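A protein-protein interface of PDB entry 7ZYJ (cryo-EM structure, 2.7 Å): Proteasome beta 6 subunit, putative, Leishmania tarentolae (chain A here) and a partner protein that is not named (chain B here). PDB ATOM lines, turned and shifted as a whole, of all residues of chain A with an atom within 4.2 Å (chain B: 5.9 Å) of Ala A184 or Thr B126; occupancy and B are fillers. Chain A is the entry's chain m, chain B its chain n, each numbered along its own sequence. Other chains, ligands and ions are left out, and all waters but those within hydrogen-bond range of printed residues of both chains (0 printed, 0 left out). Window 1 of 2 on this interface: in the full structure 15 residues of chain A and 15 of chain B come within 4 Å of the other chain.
The indole nitrogen (NE1) of Trp B128 lies close to the backbone carbonyl oxygen (O) of His A160. The side-chain amide oxygen of Gln A183 sits at hydrogen-bond distance from the backbone NH of Arg B127 (3.1 Å). The side-chain carboxylate (OD1) of Asp A185 sits at hydrogen-bond distance from the side-chain hydroxyl (OH) of Tyr B93 (3.2 Å).
N of Gln A183 sits at hydrogen-bond distance from OD1 of Asn A132 (3.0 Å). The backbone carbonyl oxygen of Gly B125 lies within hydrogen-bond range of a ring nitrogen (NE2) of His B89 (2.9 Å). The backbone NH (N) of Gly B120 sits at hydrogen-bond distance from the backbone carbonyl oxygen (O) of Trp B128.
Gln A130 touches Asp B122 (OE1 to OD2, 3.98 Å). OG1 of Thr B126 touches OE1 of Gln A130, at 3.7 Å. His A160 touches Asp B122 (NE2 to OD2, 3.8 Å). Met A182 touches Val B124 (CE to CG2, 3.5 Å). CG2 of Thr B126 touches OE1 of Gln A183, at 3.4 Å. Tyr B93 touches Ala A184. Ala A184 touches Gly B125 (CB to O, 3.3 Å). N of Thr B126 touches CB of Ala A184 (3.9 Å). Leu A187 touches Arg B127. NE2 of Gln A188 touches CE2 of Tyr B93, at 3.2 Å.
Of chain B, only Tyr B93 (3.8 Å), Gly B125 (3.3 Å) and Thr B126 (3.9 Å) come within 4 Å of Ala A184. Of the printed residues of chain A, Thr B126 touches Gln A130, Gln A183 and Ala A184. Printed residues of chain A within 4 Å of Trp B128: His A160. Printed residues of chain B within 4 Å of Gln A183: Thr B126 and Arg B127. Of the printed residues of chain B, Gln A130 touches Asp B122 (3.98 Å), Val B124 (3.5 Å) and Thr B126 (3.7 Å). Of the printed residues of chain A, Gly B125 touches Ala A184 (3.3 Å). Of the printed residues of chain B, Asp A185 touches Tyr B93 (3.2 Å). The nearest residue of chain B that does not touch Ala A184 is Val B124 (4.1 Å). The nearest printed residue of chain A that does not touch Thr B126 is Asn A132 (4.003 Å).
Of the 11 printed residues of chain B, 8 touch a printed residue of chain A. Printed residues of chain B that touch a printed residue of chain A: His B89, Tyr B93, Asp B122, Val B124, Gly B125, Thr B126, Arg B127 and Trp B128. Hydrophobic or aromatic side chains of chain B that line the printed part of chain A: His B89, Tyr B93, Val B124 and Trp B128. Printed residues of chain A that touch a printed residue of chain B: Gln A130, His A160, Met A182, Gln A183, Ala A184, Asp A185, Leu A187 and Gln A188. Hydrophobic or aromatic side chains of chain A within 4 Å of the printed part of chain B: His A160, Met A182, Ala A184 and Leu A187.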
ATOM      1  N   GLN A 130      29.786 -28.986 -19.983  1.00  0.00           N
ATOM      2  CA  GLN A 130      30.518 -29.525 -18.846  1.00  0.00           C
ATOM      3  C   GLN A 130      29.546 -30.282 -17.959  1.00  0.00           C
ATOM      4  O   GLN A 130      28.457 -29.784 -17.663  1.00  0.00           O
ATOM      5  CB  GLN A 130      31.204 -28.414 -18.043  1.00  0.00           C
ATOM      6  CG  GLN A 130      32.055 -28.922 -16.894  1.00  0.00           C
ATOM      7  CD  GLN A 130      32.763 -27.805 -16.156  1.00  0.00           C
ATOM      8  OE1 GLN A 130      32.593 -26.629 -16.477  1.00  0.00           O
ATOM      9  NE2 GLN A 130      33.561 -28.169 -15.159  1.00  0.00           N
ATOM     10  N   ASN A 132      28.777 -31.718 -14.325  1.00  0.00           N
ATOM     11  CA  ASN A 132      29.135 -31.505 -12.931  1.00  0.00           C
ATOM     12  C   ASN A 132      28.715 -32.663 -12.037  1.00  0.00           C
ATOM     13  O   ASN A 132      28.827 -32.558 -10.811  1.00  0.00           O
ATOM     14  CB  ASN A 132      28.520 -30.200 -12.427  1.00  0.00           C
ATOM     15  CG  ASN A 132      28.984 -28.995 -13.219  1.00  0.00           C
ATOM     16  OD1 ASN A 132      28.370 -28.619 -14.216  1.00  0.00           O
ATOM     17  ND2 ASN A 132      30.077 -28.383 -12.779  1.00  0.00           N
ATOM     18  N   HIS A 160      34.237 -28.336  -6.588  1.00  0.00           N
ATOM     19  CA  HIS A 160      33.880 -26.934  -6.392  1.00  0.00           C
ATOM     20  C   HIS A 160      33.273 -26.706  -5.014  1.00  0.00           C
ATOM     21  O   HIS A 160      33.682 -25.794  -4.286  1.00  0.00           O
ATOM     22  CB  HIS A 160      32.913 -26.480  -7.486  1.00  0.00           C
ATOM     23  CG  HIS A 160      33.557 -26.294  -8.823  1.00  0.00           C
ATOM     24  ND1 HIS A 160      34.907 -26.061  -8.974  1.00  0.00           N
ATOM     25  CD2 HIS A 160      33.037 -26.306 -10.072  1.00  0.00           C
ATOM     26  CE1 HIS A 160      35.190 -25.937 -10.258  1.00  0.00           C
ATOM     27  NE2 HIS A 160      34.073 -26.082 -10.946  1.00  0.00           N
ATOM     28  N   MET A 182      24.871 -30.173 -16.411  1.00  0.00           N
ATOM     29  CA  MET A 182      25.558 -28.890 -16.380  1.00  0.00           C
ATOM     30  C   MET A 182      24.873 -27.933 -15.411  1.00  0.00           C
ATOM     31  O   MET A 182      23.650 -27.772 -15.440  1.00  0.00           O
ATOM     32  CB  MET A 182      25.596 -28.294 -17.783  1.00  0.00           C
ATOM     33  CG  MET A 182      26.209 -26.923 -17.858  1.00  0.00           C
ATOM     34  SD  MET A 182      26.841 -26.578 -19.504  1.00  0.00           S
ATOM     35  CE  MET A 182      28.175 -25.475 -19.085  1.00  0.00           C
ATOM     36  N   GLN A 183      25.670 -27.298 -14.548  1.00  0.00           N
ATOM     37  CA  GLN A 183      25.112 -26.426 -13.518  1.00  0.00           C
ATOM     38  C   GLN A 183      24.638 -25.099 -14.102  1.00  0.00           C
ATOM     39  O   GLN A 183      23.556 -24.612 -13.752  1.00  0.00           O
ATOM     40  CB  GLN A 183      26.150 -26.202 -12.418  1.00  0.00           C
ATOM     41  CG  GLN A 183      25.601 -25.635 -11.120  1.00  0.00           C
ATOM     42  CD  GLN A 183      26.030 -24.206 -10.876  1.00  0.00           C
ATOM     43  OE1 GLN A 183      26.928 -23.692 -11.542  1.00  0.00           O
ATOM     44  NE2 GLN A 183      25.407 -23.563  -9.897  1.00  0.00           N
ATOM     45  N   ALA A 184      25.430 -24.502 -14.994  1.00  0.00           N
ATOM     46  CA  ALA A 184      25.031 -23.244 -15.616  1.00  0.00           C
ATOM     47  C   ALA A 184      23.775 -23.422 -16.456  1.00  0.00           C
ATOM     48  O   ALA A 184      22.887 -22.556 -16.463  1.00  0.00           O
ATOM     49  CB  ALA A 184      26.173 -22.698 -16.470  1.00  0.00           C
ATOM     50  N   ASP A 185      23.685 -24.542 -17.176  1.00  0.00           N
ATOM     51  CA  ASP A 185      22.506 -24.806 -17.988  1.00  0.00           C
ATOM     52  C   ASP A 185      21.257 -24.922 -17.126  1.00  0.00           C
ATOM     53  O   ASP A 185      20.201 -24.389 -17.483  1.00  0.00           O
ATOM     54  CB  ASP A 185      22.711 -26.072 -18.817  1.00  0.00           C
ATOM     55  CG  ASP A 185      23.381 -25.793 -20.144  1.00  0.00           C
ATOM     56  OD1 ASP A 185      23.885 -24.666 -20.331  1.00  0.00           O
ATOM     57  OD2 ASP A 185      23.402 -26.697 -21.004  1.00  0.00           O
ATOM     58  N   ARG A 186      21.352 -25.604 -15.980  1.00  0.00           N
ATOM     59  CA  ARG A 186      20.160 -25.714 -15.148  1.00  0.00           C
ATOM     60  C   ARG A 186      19.838 -24.403 -14.447  1.00  0.00           C
ATOM     61  O   ARG A 186      18.666 -24.123 -14.200  1.00  0.00           O
ATOM     62  CB  ARG A 186      20.268 -26.848 -14.126  1.00  0.00           C
ATOM     63  CG  ARG A 186      21.314 -26.730 -13.036  1.00  0.00           C
ATOM     64  CD  ARG A 186      21.229 -27.980 -12.164  1.00  0.00           C
ATOM     65  NE  ARG A 186      22.156 -27.989 -11.038  1.00  0.00           N
ATOM     66  CZ  ARG A 186      23.384 -28.484 -11.084  1.00  0.00           C
ATOM     67  NH1 ARG A 186      23.849 -29.078 -12.168  1.00  0.00           N
ATOM     68  NH2 ARG A 186      24.154 -28.406 -10.002  1.00  0.00           N
ATOM     69  N   LEU A 187      20.840 -23.580 -14.131  1.00  0.00           N
ATOM     70  CA  LEU A 187      20.537 -22.251 -13.608  1.00  0.00           C
ATOM     71  C   LEU A 187      19.754 -21.427 -14.625  1.00  0.00           C
ATOM     72  O   LEU A 187      18.736 -20.801 -14.289  1.00  0.00           O
ATOM     73  CB  LEU A 187      21.826 -21.530 -13.216  1.00  0.00           C
ATOM     74  CG  LEU A 187      22.590 -22.076 -12.008  1.00  0.00           C
ATOM     75  CD1 LEU A 187      23.928 -21.374 -11.868  1.00  0.00           C
ATOM     76  CD2 LEU A 187      21.770 -21.932 -10.739  1.00  0.00           C
ATOM     77  N   GLN A 188      20.206 -21.432 -15.881  1.00  0.00           N
ATOM     78  CA  GLN A 188      19.494 -20.710 -16.930  1.00  0.00           C
ATOM     79  C   GLN A 188      18.086 -21.264 -17.128  1.00  0.00           C
ATOM     80  O   GLN A 188      17.121 -20.500 -17.267  1.00  0.00           O
ATOM     81  CB  GLN A 188      20.289 -20.775 -18.233  1.00  0.00           C
ATOM     82  CG  GLN A 188      19.649 -20.031 -19.386  1.00  0.00           C
ATOM     83  CD  GLN A 188      19.415 -18.572 -19.066  1.00  0.00           C
ATOM     84  OE1 GLN A 188      18.289 -18.157 -18.813  1.00  0.00           O
ATOM     85  NE2 GLN A 188      20.481 -17.784 -19.073  1.00  0.00           N
ATOM     86  N   HIS B  89      28.345 -13.204 -13.480  1.00  0.00           N
ATOM     87  CA  HIS B  89      28.015 -14.559 -13.907  1.00  0.00           C
ATOM     88  C   HIS B  89      27.089 -14.553 -15.115  1.00  0.00           C
ATOM     89  O   HIS B  89      27.279 -15.334 -16.055  1.00  0.00           O
ATOM     90  CB  HIS B  89      27.386 -15.329 -12.746  1.00  0.00           C
ATOM     91  CG  HIS B  89      26.627 -16.546 -13.170  1.00  0.00           C
ATOM     92  ND1 HIS B  89      25.255 -16.563 -13.294  1.00  0.00           N
ATOM     93  CD2 HIS B  89      27.050 -17.788 -13.507  1.00  0.00           C
ATOM     94  CE1 HIS B  89      24.865 -17.764 -13.683  1.00  0.00           C
ATOM     95  NE2 HIS B  89      25.934 -18.525 -13.820  1.00  0.00           N
ATOM     96  N   TYR B  93      28.032 -16.108 -18.757  1.00  0.00           N
ATOM     97  CA  TYR B  93      27.194 -17.124 -19.383  1.00  0.00           C
ATOM     98  C   TYR B  93      26.680 -16.657 -20.738  1.00  0.00           C
ATOM     99  O   TYR B  93      26.612 -17.444 -21.690  1.00  0.00           O
ATOM    100  CB  TYR B  93      26.034 -17.489 -18.459  1.00  0.00           C
ATOM    101  CG  TYR B  93      25.155 -18.592 -19.000  1.00  0.00           C
ATOM    102  CD1 TYR B  93      25.598 -19.907 -19.023  1.00  0.00           C
ATOM    103  CD2 TYR B  93      23.886 -18.319 -19.487  1.00  0.00           C
ATOM    104  CE1 TYR B  93      24.801 -20.920 -19.516  1.00  0.00           C
ATOM    105  CE2 TYR B  93      23.083 -19.327 -19.982  1.00  0.00           C
ATOM    106  CZ  TYR B  93      23.546 -20.624 -19.994  1.00  0.00           C
ATOM    107  OH  TYR B  93      22.747 -21.630 -20.486  1.00  0.00           O
ATOM    108  N   GLY B 120      33.171 -18.164  -6.866  1.00  0.00           N
ATOM    109  CA  GLY B 120      33.986 -18.433  -8.035  1.00  0.00           C
ATOM    110  C   GLY B 120      33.109 -18.740  -9.228  1.00  0.00           C
ATOM    111  O   GLY B 120      32.003 -19.272  -9.093  1.00  0.00           O
ATOM    112  N   VAL B 121      33.616 -18.390 -10.409  1.00  0.00           N
ATOM    113  CA  VAL B 121      32.887 -18.572 -11.660  1.00  0.00           C
ATOM    114  C   VAL B 121      33.850 -19.052 -12.741  1.00  0.00           C
ATOM    115  O   VAL B 121      34.996 -18.601 -12.814  1.00  0.00           O
ATOM    116  CB  VAL B 121      32.160 -17.275 -12.080  1.00  0.00           C
ATOM    117  CG1 VAL B 121      33.149 -16.152 -12.348  1.00  0.00           C
ATOM    118  CG2 VAL B 121      31.271 -17.520 -13.290  1.00  0.00           C
ATOM    119  N   ASP B 122      33.382 -19.984 -13.573  1.00  0.00           N
ATOM    120  CA  ASP B 122      34.157 -20.512 -14.686  1.00  0.00           C
ATOM    121  C   ASP B 122      33.939 -19.693 -15.955  1.00  0.00           C
ATOM    122  O   ASP B 122      33.131 -18.764 -16.005  1.00  0.00           O
ATOM    123  CB  ASP B 122      33.808 -21.977 -14.949  1.00  0.00           C
ATOM    124  CG  ASP B 122      34.268 -22.891 -13.845  1.00  0.00           C
ATOM    125  OD1 ASP B 122      34.388 -22.418 -12.703  1.00  0.00           O
ATOM    126  OD2 ASP B 122      34.549 -24.074 -14.127  1.00  0.00           O
ATOM    127  N   ASP B 123      34.677 -20.060 -17.002  1.00  0.00           N
ATOM    128  CA  ASP B 123      34.547 -19.438 -18.311  1.00  0.00           C
ATOM    129  C   ASP B 123      33.296 -19.879 -19.053  1.00  0.00           C
ATOM    130  O   ASP B 123      32.962 -19.282 -20.082  1.00  0.00           O
ATOM    131  CB  ASP B 123      35.775 -19.756 -19.165  1.00  0.00           C
ATOM    132  CG  ASP B 123      36.064 -21.240 -19.234  1.00  0.00           C
ATOM    133  OD1 ASP B 123      36.151 -21.881 -18.166  1.00  0.00           O
ATOM    134  OD2 ASP B 123      36.207 -21.766 -20.358  1.00  0.00           O
ATOM    135  N   VAL B 124      32.603 -20.909 -18.567  1.00  0.00           N
ATOM    136  CA  VAL B 124      31.450 -21.448 -19.274  1.00  0.00           C
ATOM    137  C   VAL B 124      30.145 -21.158 -18.538  1.00  0.00           C
ATOM    138  O   VAL B 124      29.063 -21.463 -19.064  1.00  0.00           O
ATOM    139  CB  VAL B 124      31.630 -22.967 -19.509  1.00  0.00           C
ATOM    140  CG1 VAL B 124      31.635 -23.735 -18.188  1.00  0.00           C
ATOM    141  CG2 VAL B 124      30.646 -23.518 -20.533  1.00  0.00           C
ATOM    142  N   GLY B 125      30.210 -20.549 -17.354  1.00  0.00           N
ATOM    143  CA  GLY B 125      29.026 -20.139 -16.624  1.00  0.00           C
ATOM    144  C   GLY B 125      28.811 -20.827 -15.295  1.00  0.00           C
ATOM    145  O   GLY B 125      27.840 -20.499 -14.605  1.00  0.00           O
ATOM    146  N   THR B 126      29.667 -21.769 -14.911  1.00  0.00           N
ATOM    147  CA  THR B 126      29.524 -22.416 -13.614  1.00  0.00           C
ATOM    148  C   THR B 126      29.868 -21.433 -12.504  1.00  0.00           C
ATOM    149  O   THR B 126      30.871 -20.722 -12.583  1.00  0.00           O
ATOM    150  CB  THR B 126      30.426 -23.646 -13.529  1.00  0.00           C
ATOM    151  OG1 THR B 126      30.177 -24.501 -14.651  1.00  0.00           O
ATOM    152  CG2 THR B 126      30.159 -24.416 -12.249  1.00  0.00           C
ATOM    153  N   ARG B 127      29.033 -21.390 -11.469  1.00  0.00           N
ATOM    154  CA  ARG B 127      29.243 -20.510 -10.330  1.00  0.00           C
ATOM    155  C   ARG B 127      29.052 -21.294  -9.040  1.00  0.00           C
ATOM    156  O   ARG B 127      28.258 -22.236  -8.981  1.00  0.00           O
ATOM    157  CB  ARG B 127      28.286 -19.304 -10.360  1.00  0.00           C
ATOM    158  CG  ARG B 127      26.884 -19.607  -9.853  1.00  0.00           C
ATOM    159  CD  ARG B 127      25.913 -18.481 -10.158  1.00  0.00           C
ATOM    160  NE  ARG B 127      26.083 -17.341  -9.264  1.00  0.00           N
ATOM    161  CZ  ARG B 127      25.604 -17.280  -8.029  1.00  0.00           C
ATOM    162  NH1 ARG B 127      24.928 -18.286  -7.500  1.00  0.00           N
ATOM    163  NH2 ARG B 127      25.807 -16.183  -7.308  1.00  0.00           N
ATOM    164  N   TRP B 128      29.802 -20.910  -8.010  1.00  0.00           N
ATOM    165  CA  TRP B 128      29.618 -21.522  -6.701  1.00  0.00           C
ATOM    166  C   TRP B 128      30.124 -20.578  -5.621  1.00  0.00           C
ATOM    167  O   TRP B 128      30.908 -19.665  -5.883  1.00  0.00           O
ATOM    168  CB  TRP B 128      30.326 -22.879  -6.594  1.00  0.00           C
ATOM    169  CG  TRP B 128      31.813 -22.799  -6.640  1.00  0.00           C
ATOM    170  CD1 TRP B 128      32.671 -22.902  -5.587  1.00  0.00           C
ATOM    171  CD2 TRP B 128      32.623 -22.577  -7.796  1.00  0.00           C
ATOM    172  NE1 TRP B 128      33.968 -22.774  -6.018  1.00  0.00           N
ATOM    173  CE2 TRP B 128      33.965 -22.570  -7.371  1.00  0.00           C
ATOM    174  CE3 TRP B 128      32.345 -22.391  -9.151  1.00  0.00           C
ATOM    175  CZ2 TRP B 128      35.023 -22.380  -8.251  1.00  0.00           C
ATOM    176  CZ3 TRP B 128      33.390 -22.202 -10.017  1.00  0.00           C
ATOM    177  CH2 TRP B 128      34.715 -22.199  -9.569  1.00  0.00           C
